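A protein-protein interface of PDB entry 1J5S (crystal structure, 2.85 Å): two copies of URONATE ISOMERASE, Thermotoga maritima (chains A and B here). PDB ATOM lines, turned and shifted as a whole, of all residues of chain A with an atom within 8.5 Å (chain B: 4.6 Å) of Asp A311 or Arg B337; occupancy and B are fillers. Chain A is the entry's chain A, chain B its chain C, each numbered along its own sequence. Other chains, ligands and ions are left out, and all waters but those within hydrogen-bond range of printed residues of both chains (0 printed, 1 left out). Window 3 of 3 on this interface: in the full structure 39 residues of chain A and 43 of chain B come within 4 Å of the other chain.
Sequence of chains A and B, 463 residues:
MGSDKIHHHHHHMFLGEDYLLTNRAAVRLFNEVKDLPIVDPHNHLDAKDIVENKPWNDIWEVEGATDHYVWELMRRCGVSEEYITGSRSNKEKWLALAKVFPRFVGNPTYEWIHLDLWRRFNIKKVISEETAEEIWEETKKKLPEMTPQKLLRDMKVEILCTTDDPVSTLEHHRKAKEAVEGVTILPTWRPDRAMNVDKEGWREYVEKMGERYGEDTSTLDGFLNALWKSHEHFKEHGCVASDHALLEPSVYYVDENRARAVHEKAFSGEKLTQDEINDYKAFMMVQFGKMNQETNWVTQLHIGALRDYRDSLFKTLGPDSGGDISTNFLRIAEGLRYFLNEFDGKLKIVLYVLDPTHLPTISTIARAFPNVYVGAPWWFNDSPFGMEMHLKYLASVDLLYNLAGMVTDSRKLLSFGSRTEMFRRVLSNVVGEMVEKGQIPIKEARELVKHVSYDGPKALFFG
O of Asp A308 is in hydrogen-bond range of NH2 of Arg B337, 3.2 Å away. N of Arg B337 sits at hydrogen-bond distance from OH of Tyr A309 (3.1 Å). The backbone carbonyl oxygen (O) of Tyr A309 lies within hydrogen-bond range of the side-chain amide nitrogen (ND2) of Asn B341 (3.1 Å). The guanidinium group (NH2) of Arg B337 is in salt-bridge range of the side-chain carboxylate (OD1) of Asp A311, at 3.4 Å. N of Asp A311 lies within hydrogen-bond range of OD1 of Asn B341 (2.6 Å). The side-chain hydroxyl (OH) of Tyr A309 sits close to the backbone carbonyl oxygen (O) of Ala B333 (2.3 Å).
No position is printed for both chains. Of the 12 pairs that touch across the chains among the printed residues, none has its exchanged pair printed and touching as well.
Among the printed residues, pairs that only touch across the chains: Leu A306 with Glu B334 (3.2 Å), Arg A310 with Asn B341 (3.5 Å), Tyr A309 with Leu B336 (3.7 Å), Ile A325 with Ala B333 (3.8 Å), Tyr A309 with Leu B340 (3.9 Å) and Leu A306 with Ala B333 (3.9 Å).
N of Leu A306 is in hydrogen-bond range of O of Ile A325 (2.9 Å). O of Gly A323 sits at hydrogen-bond distance from N of Tyr A309 (2.9 Å). N of Arg A310 sits at hydrogen-bond distance from O of Gly A323, at 3.4 Å. The guanidinium group of Arg B337 lies within salt-bridge range of the side-chain carboxylate of Glu B334. O of Arg B337 lies within hydrogen-bond range of ND2 of Asn B341 (2.7 Å).
Of the printed residues of chain B, Asp A308 touches Arg B337. Of the printed residues of chain B, Tyr A309 touches Ala B333 (2.3 Å), Leu B336 (3.7 Å), Arg B337 (3.1 Å), Leu B340 (3.9 Å) and Asn B341 (3.1 Å). Asp A311 touches just these residues of chain B: Arg B337 (3.4 Å) and Asn B341 (2.6 Å). Of the printed residues of chain A, Ala B333 touches Leu A306 (3.9 Å), Tyr A309 (2.3 Å) and Ile A325 (3.8 Å). No residue of chain A comes within 4 Å of Gly B335. Of the printed residues of chain A, Arg B337 touches Asp A308 (3.2 Å), Tyr A309 (3.1 Å) and Asp A311 (3.4 Å). Printed residues of chain A within 4 Å of Leu B340: Tyr A309 (3.9 Å). The nearest printed residue of chain B that does not touch Asp A308 is Asn B341 (6.0 Å).
Of the 9 printed residues of chain B, 6 touch a printed residue of chain A. Along chain B the printed residues that touch a printed residue of chain A span positions 333 to 341. Of the 18 printed residues of chain A, 6 touch a printed residue of chain B. Hydrophobic or aromatic side chains of chain A that line the printed part of chain B: Leu A306, Tyr A309 and Ile A325. Among the printed residues, 12 pairs touch across the chains.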
ATOM      1  N   LEU A 247      24.204  -8.015  -2.715  1.00  0.00           N
ATOM      2  CA  LEU A 247      23.311  -7.834  -3.838  1.00  0.00           C
ATOM      3  C   LEU A 247      24.057  -8.171  -5.117  1.00  0.00           C
ATOM      4  O   LEU A 247      23.676  -9.075  -5.856  1.00  0.00           O
ATOM      5  CB  LEU A 247      22.818  -6.391  -3.881  1.00  0.00           C
ATOM      6  CG  LEU A 247      21.690  -6.147  -4.876  1.00  0.00           C
ATOM      7  CD1 LEU A 247      20.431  -6.854  -4.417  1.00  0.00           C
ATOM      8  CD2 LEU A 247      21.445  -4.662  -5.037  1.00  0.00           C
ATOM      9  N   LEU A 306      17.450  -7.494  -2.906  1.00  0.00           N
ATOM     10  CA  LEU A 306      17.286  -6.049  -2.928  1.00  0.00           C
ATOM     11  C   LEU A 306      16.448  -5.761  -1.702  1.00  0.00           C
ATOM     12  O   LEU A 306      15.321  -6.235  -1.596  1.00  0.00           O
ATOM     13  CB  LEU A 306      16.517  -5.588  -4.157  1.00  0.00           C
ATOM     14  CG  LEU A 306      17.217  -4.639  -5.130  1.00  0.00           C
ATOM     15  CD1 LEU A 306      16.225  -4.231  -6.220  1.00  0.00           C
ATOM     16  CD2 LEU A 306      17.780  -3.412  -4.423  1.00  0.00           C
ATOM     17  N   ARG A 307      16.957  -4.983  -0.768  1.00  0.00           N
ATOM     18  CA  ARG A 307      16.226  -4.851   0.476  1.00  0.00           C
ATOM     19  C   ARG A 307      15.648  -3.486   0.702  1.00  0.00           C
ATOM     20  O   ARG A 307      16.179  -2.481   0.236  1.00  0.00           O
ATOM     21  CB  ARG A 307      17.119  -5.231   1.632  1.00  0.00           C
ATOM     22  CG  ARG A 307      17.805  -6.530   1.352  1.00  0.00           C
ATOM     23  CD  ARG A 307      18.819  -6.924   2.358  1.00  0.00           C
ATOM     24  NE  ARG A 307      19.023  -8.363   2.295  1.00  0.00           N
ATOM     25  CZ  ARG A 307      19.422  -9.115   3.313  1.00  0.00           C
ATOM     26  NH1 ARG A 307      19.677  -8.562   4.497  1.00  0.00           N
ATOM     27  NH2 ARG A 307      19.571 -10.429   3.146  1.00  0.00           N
ATOM     28  N   ASP A 308      14.541  -3.470   1.423  1.00  0.00           N
ATOM     29  CA  ASP A 308      13.888  -2.236   1.758  1.00  0.00           C
ATOM     30  C   ASP A 308      13.552  -1.514   0.470  1.00  0.00           C
ATOM     31  O   ASP A 308      13.703  -0.299   0.352  1.00  0.00           O
ATOM     32  CB  ASP A 308      14.771  -1.418   2.681  1.00  0.00           C
ATOM     33  CG  ASP A 308      15.070  -2.144   3.972  1.00  0.00           C
ATOM     34  OD1 ASP A 308      14.324  -3.085   4.327  1.00  0.00           O
ATOM     35  OD2 ASP A 308      16.032  -1.833   4.701  1.00  0.00           O
ATOM     36  N   TYR A 309      13.090  -2.293  -0.495  1.00  0.00           N
ATOM     37  CA  TYR A 309      12.689  -1.766  -1.781  1.00  0.00           C
ATOM     38  C   TYR A 309      11.437  -0.918  -1.565  1.00  0.00           C
ATOM     39  O   TYR A 309      11.319   0.171  -2.105  1.00  0.00           O
ATOM     40  CB  TYR A 309      12.467  -2.938  -2.737  1.00  0.00           C
ATOM     41  CG  TYR A 309      12.125  -2.585  -4.158  1.00  0.00           C
ATOM     42  CD1 TYR A 309      13.099  -2.525  -5.134  1.00  0.00           C
ATOM     43  CD2 TYR A 309      10.823  -2.374  -4.533  1.00  0.00           C
ATOM     44  CE1 TYR A 309      12.775  -2.235  -6.448  1.00  0.00           C
ATOM     45  CE2 TYR A 309      10.494  -2.086  -5.826  1.00  0.00           C
ATOM     46  CZ  TYR A 309      11.471  -2.014  -6.778  1.00  0.00           C
ATOM     47  OH  TYR A 309      11.128  -1.727  -8.062  1.00  0.00           O
ATOM     48  N   ARG A 310      10.531  -1.407  -0.731  1.00  0.00           N
ATOM     49  CA  ARG A 310       9.324  -0.658  -0.407  1.00  0.00           C
ATOM     50  C   ARG A 310       9.509   0.332   0.744  1.00  0.00           C
ATOM     51  O   ARG A 310       9.538  -0.052   1.910  1.00  0.00           O
ATOM     52  CB  ARG A 310       8.204  -1.608  -0.064  1.00  0.00           C
ATOM     53  CG  ARG A 310       6.896  -0.935  -0.087  1.00  0.00           C
ATOM     54  CD  ARG A 310       5.803  -1.911  -0.118  1.00  0.00           C
ATOM     55  NE  ARG A 310       4.543  -1.286   0.218  1.00  0.00           N
ATOM     56  CZ  ARG A 310       3.620  -1.846   0.965  1.00  0.00           C
ATOM     57  NH1 ARG A 310       3.808  -3.061   1.458  1.00  0.00           N
ATOM     58  NH2 ARG A 310       2.508  -1.189   1.217  1.00  0.00           N
ATOM     59  N   ASP A 311       9.576   1.609   0.394  1.00  0.00           N
ATOM     60  CA  ASP A 311       9.841   2.684   1.341  1.00  0.00           C
ATOM     61  C   ASP A 311       8.925   2.733   2.541  1.00  0.00           C
ATOM     62  O   ASP A 311       9.386   2.859   3.667  1.00  0.00           O
ATOM     63  CB  ASP A 311       9.710   4.042   0.653  1.00  0.00           C
ATOM     64  CG  ASP A 311      10.563   4.165  -0.605  1.00  0.00           C
ATOM     65  OD1 ASP A 311      11.236   3.172  -1.003  1.00  0.00           O
ATOM     66  OD2 ASP A 311      10.602   5.234  -1.266  1.00  0.00           O
ATOM     67  N   SER A 312       7.624   2.674   2.306  1.00  0.00           N
ATOM     68  CA  SER A 312       6.666   2.880   3.380  1.00  0.00           C
ATOM     69  C   SER A 312       6.878   1.855   4.462  1.00  0.00           C
ATOM     70  O   SER A 312       6.656   2.117   5.640  1.00  0.00           O
ATOM     71  CB  SER A 312       5.239   2.798   2.848  1.00  0.00           C
ATOM     72  OG  SER A 312       4.957   1.505   2.337  1.00  0.00           O
ATOM     73  N   LEU A 313       7.314   0.679   4.047  1.00  0.00           N
ATOM     74  CA  LEU A 313       7.527  -0.417   4.958  1.00  0.00           C
ATOM     75  C   LEU A 313       8.795  -0.118   5.740  1.00  0.00           C
ATOM     76  O   LEU A 313       8.902  -0.425   6.919  1.00  0.00           O
ATOM     77  CB  LEU A 313       7.652  -1.717   4.148  1.00  0.00           C
ATOM     78  CG  LEU A 313       7.053  -3.027   4.674  1.00  0.00           C
ATOM     79  CD1 LEU A 313       5.884  -2.818   5.620  1.00  0.00           C
ATOM     80  CD2 LEU A 313       6.614  -3.861   3.501  1.00  0.00           C
ATOM     81  N   PHE A 314       9.746   0.519   5.080  1.00  0.00           N
ATOM     82  CA  PHE A 314      11.017   0.800   5.712  1.00  0.00           C
ATOM     83  C   PHE A 314      10.835   1.850   6.798  1.00  0.00           C
ATOM     84  O   PHE A 314      11.173   1.632   7.960  1.00  0.00           O
ATOM     85  CB  PHE A 314      12.052   1.262   4.691  1.00  0.00           C
ATOM     86  CG  PHE A 314      13.413   1.387   5.273  1.00  0.00           C
ATOM     87  CD1 PHE A 314      14.100   0.256   5.673  1.00  0.00           C
ATOM     88  CD2 PHE A 314      13.980   2.627   5.490  1.00  0.00           C
ATOM     89  CE1 PHE A 314      15.348   0.355   6.251  1.00  0.00           C
ATOM     90  CE2 PHE A 314      15.232   2.738   6.065  1.00  0.00           C
ATOM     91  CZ  PHE A 314      15.919   1.597   6.445  1.00  0.00           C
ATOM     92  N   LYS A 315      10.256   2.977   6.412  1.00  0.00           N
ATOM     93  CA  LYS A 315      10.037   4.089   7.321  1.00  0.00           C
ATOM     94  C   LYS A 315       9.135   3.730   8.484  1.00  0.00           C
ATOM     95  O   LYS A 315       9.171   4.370   9.527  1.00  0.00           O
ATOM     96  CB  LYS A 315       9.400   5.237   6.557  1.00  0.00           C
ATOM     97  CG  LYS A 315      10.210   5.683   5.362  1.00  0.00           C
ATOM     98  CD  LYS A 315       9.739   7.035   4.916  1.00  0.00           C
ATOM     99  CE  LYS A 315      10.550   7.577   3.767  1.00  0.00           C
ATOM    100  NZ  LYS A 315       9.928   8.844   3.264  1.00  0.00           N
ATOM    101  N   THR A 316       8.330   2.697   8.301  1.00  0.00           N
ATOM    102  CA  THR A 316       7.326   2.326   9.283  1.00  0.00           C
ATOM    103  C   THR A 316       7.779   1.185  10.194  1.00  0.00           C
ATOM    104  O   THR A 316       7.805   1.333  11.416  1.00  0.00           O
ATOM    105  CB  THR A 316       6.036   1.971   8.516  1.00  0.00           C
ATOM    106  OG1 THR A 316       5.443   3.174   8.004  1.00  0.00           O
ATOM    107  CG2 THR A 316       4.970   1.390   9.414  1.00  0.00           C
ATOM    108  N   LEU A 317       8.135   0.051   9.604  1.00  0.00           N
ATOM    109  CA  LEU A 317       8.602  -1.083  10.386  1.00  0.00           C
ATOM    110  C   LEU A 317      10.114  -1.279  10.264  1.00  0.00           C
ATOM    111  O   LEU A 317      10.737  -1.902  11.132  1.00  0.00           O
ATOM    112  CB  LEU A 317       7.887  -2.354   9.939  1.00  0.00           C
ATOM    113  CG  LEU A 317       6.365  -2.275  10.006  1.00  0.00           C
ATOM    114  CD1 LEU A 317       5.733  -3.509   9.385  1.00  0.00           C
ATOM    115  CD2 LEU A 317       5.901  -2.092  11.448  1.00  0.00           C
ATOM    116  N   GLY A 318      10.699  -0.743   9.192  1.00  0.00           N
ATOM    117  CA  GLY A 318      12.114  -0.934   8.921  1.00  0.00           C
ATOM    118  C   GLY A 318      12.398  -2.276   8.261  1.00  0.00           C
ATOM    119  O   GLY A 318      11.522  -2.888   7.662  1.00  0.00           O
ATOM    120  N   PRO A 319      13.638  -2.729   8.387  1.00  0.00           N
ATOM    121  CA  PRO A 319      14.113  -3.973   7.765  1.00  0.00           C
ATOM    122  C   PRO A 319      13.368  -5.267   8.099  1.00  0.00           C
ATOM    123  O   PRO A 319      12.750  -5.401   9.155  1.00  0.00           O
ATOM    124  CB  PRO A 319      15.564  -4.071   8.264  1.00  0.00           C
ATOM    125  CG  PRO A 319      15.950  -2.692   8.641  1.00  0.00           C
ATOM    126  CD  PRO A 319      14.707  -2.035   9.125  1.00  0.00           C
ATOM    127  N   SER A 321      10.666  -6.516   7.039  1.00  0.00           N
ATOM    128  CA  SER A 321       9.296  -6.263   7.424  1.00  0.00           C
ATOM    129  C   SER A 321       8.333  -6.607   6.307  1.00  0.00           C
ATOM    130  O   SER A 321       7.124  -6.404   6.448  1.00  0.00           O
ATOM    131  CB  SER A 321       9.164  -4.804   7.860  1.00  0.00           C
ATOM    132  OG  SER A 321       9.290  -3.921   6.765  1.00  0.00           O
ATOM    133  N   GLY A 323       9.334  -6.029   2.642  1.00  0.00           N
ATOM    134  CA  GLY A 323       9.581  -5.240   1.444  1.00  0.00           C
ATOM    135  C   GLY A 323      10.887  -5.483   0.701  1.00  0.00           C
ATOM    136  O   GLY A 323      11.433  -4.564   0.086  1.00  0.00           O
ATOM    137  N   ILE A 325      12.879  -7.675  -2.305  1.00  0.00           N
ATOM    138  CA  ILE A 325      12.561  -8.390  -3.516  1.00  0.00           C
ATOM    139  C   ILE A 325      13.833  -8.896  -4.141  1.00  0.00           C
ATOM    140  O   ILE A 325      14.927  -8.575  -3.683  1.00  0.00           O
ATOM    141  CB  ILE A 325      11.798  -7.501  -4.513  1.00  0.00           C
ATOM    142  CG1 ILE A 325      12.721  -6.423  -5.081  1.00  0.00           C
ATOM    143  CG2 ILE A 325      10.582  -6.876  -3.845  1.00  0.00           C
ATOM    144  CD1 ILE A 325      12.124  -5.657  -6.241  1.00  0.00           C
ATOM    145  N   ALA B 333      13.547  -4.060 -11.757  1.00  0.00           N
ATOM    146  CA  ALA B 333      13.303  -3.629 -10.388  1.00  0.00           C
ATOM    147  C   ALA B 333      13.714  -2.205 -10.078  1.00  0.00           C
ATOM    148  O   ALA B 333      12.946  -1.436  -9.502  1.00  0.00           O
ATOM    149  CB  ALA B 333      13.984  -4.576  -9.427  1.00  0.00           C
ATOM    150  N   GLU B 334      14.926  -1.837 -10.435  1.00  0.00           N
ATOM    151  CA  GLU B 334      15.376  -0.512 -10.052  1.00  0.00           C
ATOM    152  C   GLU B 334      14.714   0.541 -10.940  1.00  0.00           C
ATOM    153  O   GLU B 334      14.590   1.703 -10.552  1.00  0.00           O
ATOM    154  CB  GLU B 334      16.900  -0.445  -9.986  1.00  0.00           C
ATOM    155  CG  GLU B 334      17.423  -1.116  -8.705  1.00  0.00           C
ATOM    156  CD  GLU B 334      17.067  -0.350  -7.419  1.00  0.00           C
ATOM    157  OE1 GLU B 334      16.848  -1.005  -6.362  1.00  0.00           O
ATOM    158  OE2 GLU B 334      17.008   0.911  -7.453  1.00  0.00           O
ATOM    159  N   GLY B 335      14.230   0.115 -12.103  1.00  0.00           N
ATOM    160  CA  GLY B 335      13.484   0.997 -12.988  1.00  0.00           C
ATOM    161  C   GLY B 335      12.039   1.259 -12.574  1.00  0.00           C
ATOM    162  O   GLY B 335      11.482   2.300 -12.893  1.00  0.00           O
ATOM    163  N   LEU B 336      11.415   0.332 -11.857  1.00  0.00           N
ATOM    164  CA  LEU B 336      10.017   0.517 -11.460  1.00  0.00           C
ATOM    165  C   LEU B 336       9.921   1.117 -10.085  1.00  0.00           C
ATOM    166  O   LEU B 336       8.879   1.634  -9.682  1.00  0.00           O
ATOM    167  CB  LEU B 336       9.289  -0.818 -11.443  1.00  0.00           C
ATOM    168  CG  LEU B 336       9.017  -1.368 -12.830  1.00  0.00           C
ATOM    169  CD1 LEU B 336       8.621  -2.815 -12.753  1.00  0.00           C
ATOM    170  CD2 LEU B 336       7.925  -0.551 -13.512  1.00  0.00           C
ATOM    171  N   ARG B 337      11.033   1.045  -9.376  1.00  0.00           N
ATOM    172  CA  ARG B 337      11.077   1.398  -7.981  1.00  0.00           C
ATOM    173  C   ARG B 337      10.475   2.744  -7.608  1.00  0.00           C
ATOM    174  O   ARG B 337       9.740   2.858  -6.630  1.00  0.00           O
ATOM    175  CB  ARG B 337      12.512   1.372  -7.574  1.00  0.00           C
ATOM    176  CG  ARG B 337      12.712   2.050  -6.323  1.00  0.00           C
ATOM    177  CD  ARG B 337      13.988   1.711  -5.674  1.00  0.00           C
ATOM    178  NE  ARG B 337      13.813   2.020  -4.274  1.00  0.00           N
ATOM    179  CZ  ARG B 337      14.373   1.369  -3.289  1.00  0.00           C
ATOM    180  NH1 ARG B 337      15.212   0.362  -3.535  1.00  0.00           N
ATOM    181  NH2 ARG B 337      14.099   1.751  -2.051  1.00  0.00           N
ATOM    182  N   TYR B 338      10.785   3.766  -8.383  1.00  0.00           N
ATOM    183  CA  TYR B 338      10.291   5.090  -8.098  1.00  0.00           C
ATOM    184  C   TYR B 338       8.783   5.121  -8.259  1.00  0.00           C
ATOM    185  O   TYR B 338       8.055   5.551  -7.368  1.00  0.00           O
ATOM    186  CB  TYR B 338      10.928   6.103  -9.041  1.00  0.00           C
ATOM    187  CG  TYR B 338      10.506   7.488  -8.690  1.00  0.00           C
ATOM    188  CD1 TYR B 338      11.043   8.123  -7.595  1.00  0.00           C
ATOM    189  CD2 TYR B 338       9.521   8.140  -9.410  1.00  0.00           C
ATOM    190  CE1 TYR B 338      10.636   9.382  -7.241  1.00  0.00           C
ATOM    191  CE2 TYR B 338       9.106   9.393  -9.063  1.00  0.00           C
ATOM    192  CZ  TYR B 338       9.670  10.009  -7.979  1.00  0.00           C
ATOM    193  OH  TYR B 338       9.257  11.260  -7.621  1.00  0.00           O
ATOM    194  N   PHE B 339       8.335   4.655  -9.412  1.00  0.00           N
ATOM    195  CA  PHE B 339       6.930   4.603  -9.750  1.00  0.00           C
ATOM    196  C   PHE B 339       6.183   3.883  -8.642  1.00  0.00           C
ATOM    197  O   PHE B 339       5.214   4.394  -8.072  1.00  0.00           O
ATOM    198  CB  PHE B 339       6.807   3.825 -11.074  1.00  0.00           C
ATOM    199  CG  PHE B 339       5.440   3.842 -11.708  1.00  0.00           C
ATOM    200  CD1 PHE B 339       5.071   4.852 -12.578  1.00  0.00           C
ATOM    201  CD2 PHE B 339       4.560   2.802 -11.503  1.00  0.00           C
ATOM    202  CE1 PHE B 339       3.835   4.845 -13.186  1.00  0.00           C
ATOM    203  CE2 PHE B 339       3.317   2.798 -12.115  1.00  0.00           C
ATOM    204  CZ  PHE B 339       2.958   3.822 -12.950  1.00  0.00           C
ATOM    205  N   LEU B 340       6.672   2.696  -8.317  1.00  0.00           N
ATOM    206  CA  LEU B 340       5.976   1.803  -7.411  1.00  0.00           C
ATOM    207  C   LEU B 340       5.878   2.365  -6.001  1.00  0.00           C
ATOM    208  O   LEU B 340       4.860   2.206  -5.324  1.00  0.00           O
ATOM    209  CB  LEU B 340       6.670   0.433  -7.417  1.00  0.00           C
ATOM    210  CG  LEU B 340       6.323  -0.505  -8.589  1.00  0.00           C
ATOM    211  CD1 LEU B 340       7.290  -1.647  -8.649  1.00  0.00           C
ATOM    212  CD2 LEU B 340       4.948  -1.064  -8.444  1.00  0.00           C
ATOM    213  N   ASN B 341       6.929   3.036  -5.560  1.00  0.00           N
ATOM    214  CA  ASN B 341       6.922   3.573  -4.217  1.00  0.00           C
ATOM    215  C   ASN B 341       6.079   4.798  -4.205  1.00  0.00           C
ATOM    216  O   ASN B 341       5.499   5.183  -3.184  1.00  0.00           O
ATOM    217  CB  ASN B 341       8.318   3.909  -3.759  1.00  0.00           C
ATOM    218  CG  ASN B 341       9.014   2.721  -3.203  1.00  0.00           C
ATOM    219  OD1 ASN B 341       8.901   2.430  -2.022  1.00  0.00           O
ATOM    220  ND2 ASN B 341       9.694   1.986  -4.058  1.00  0.00           N
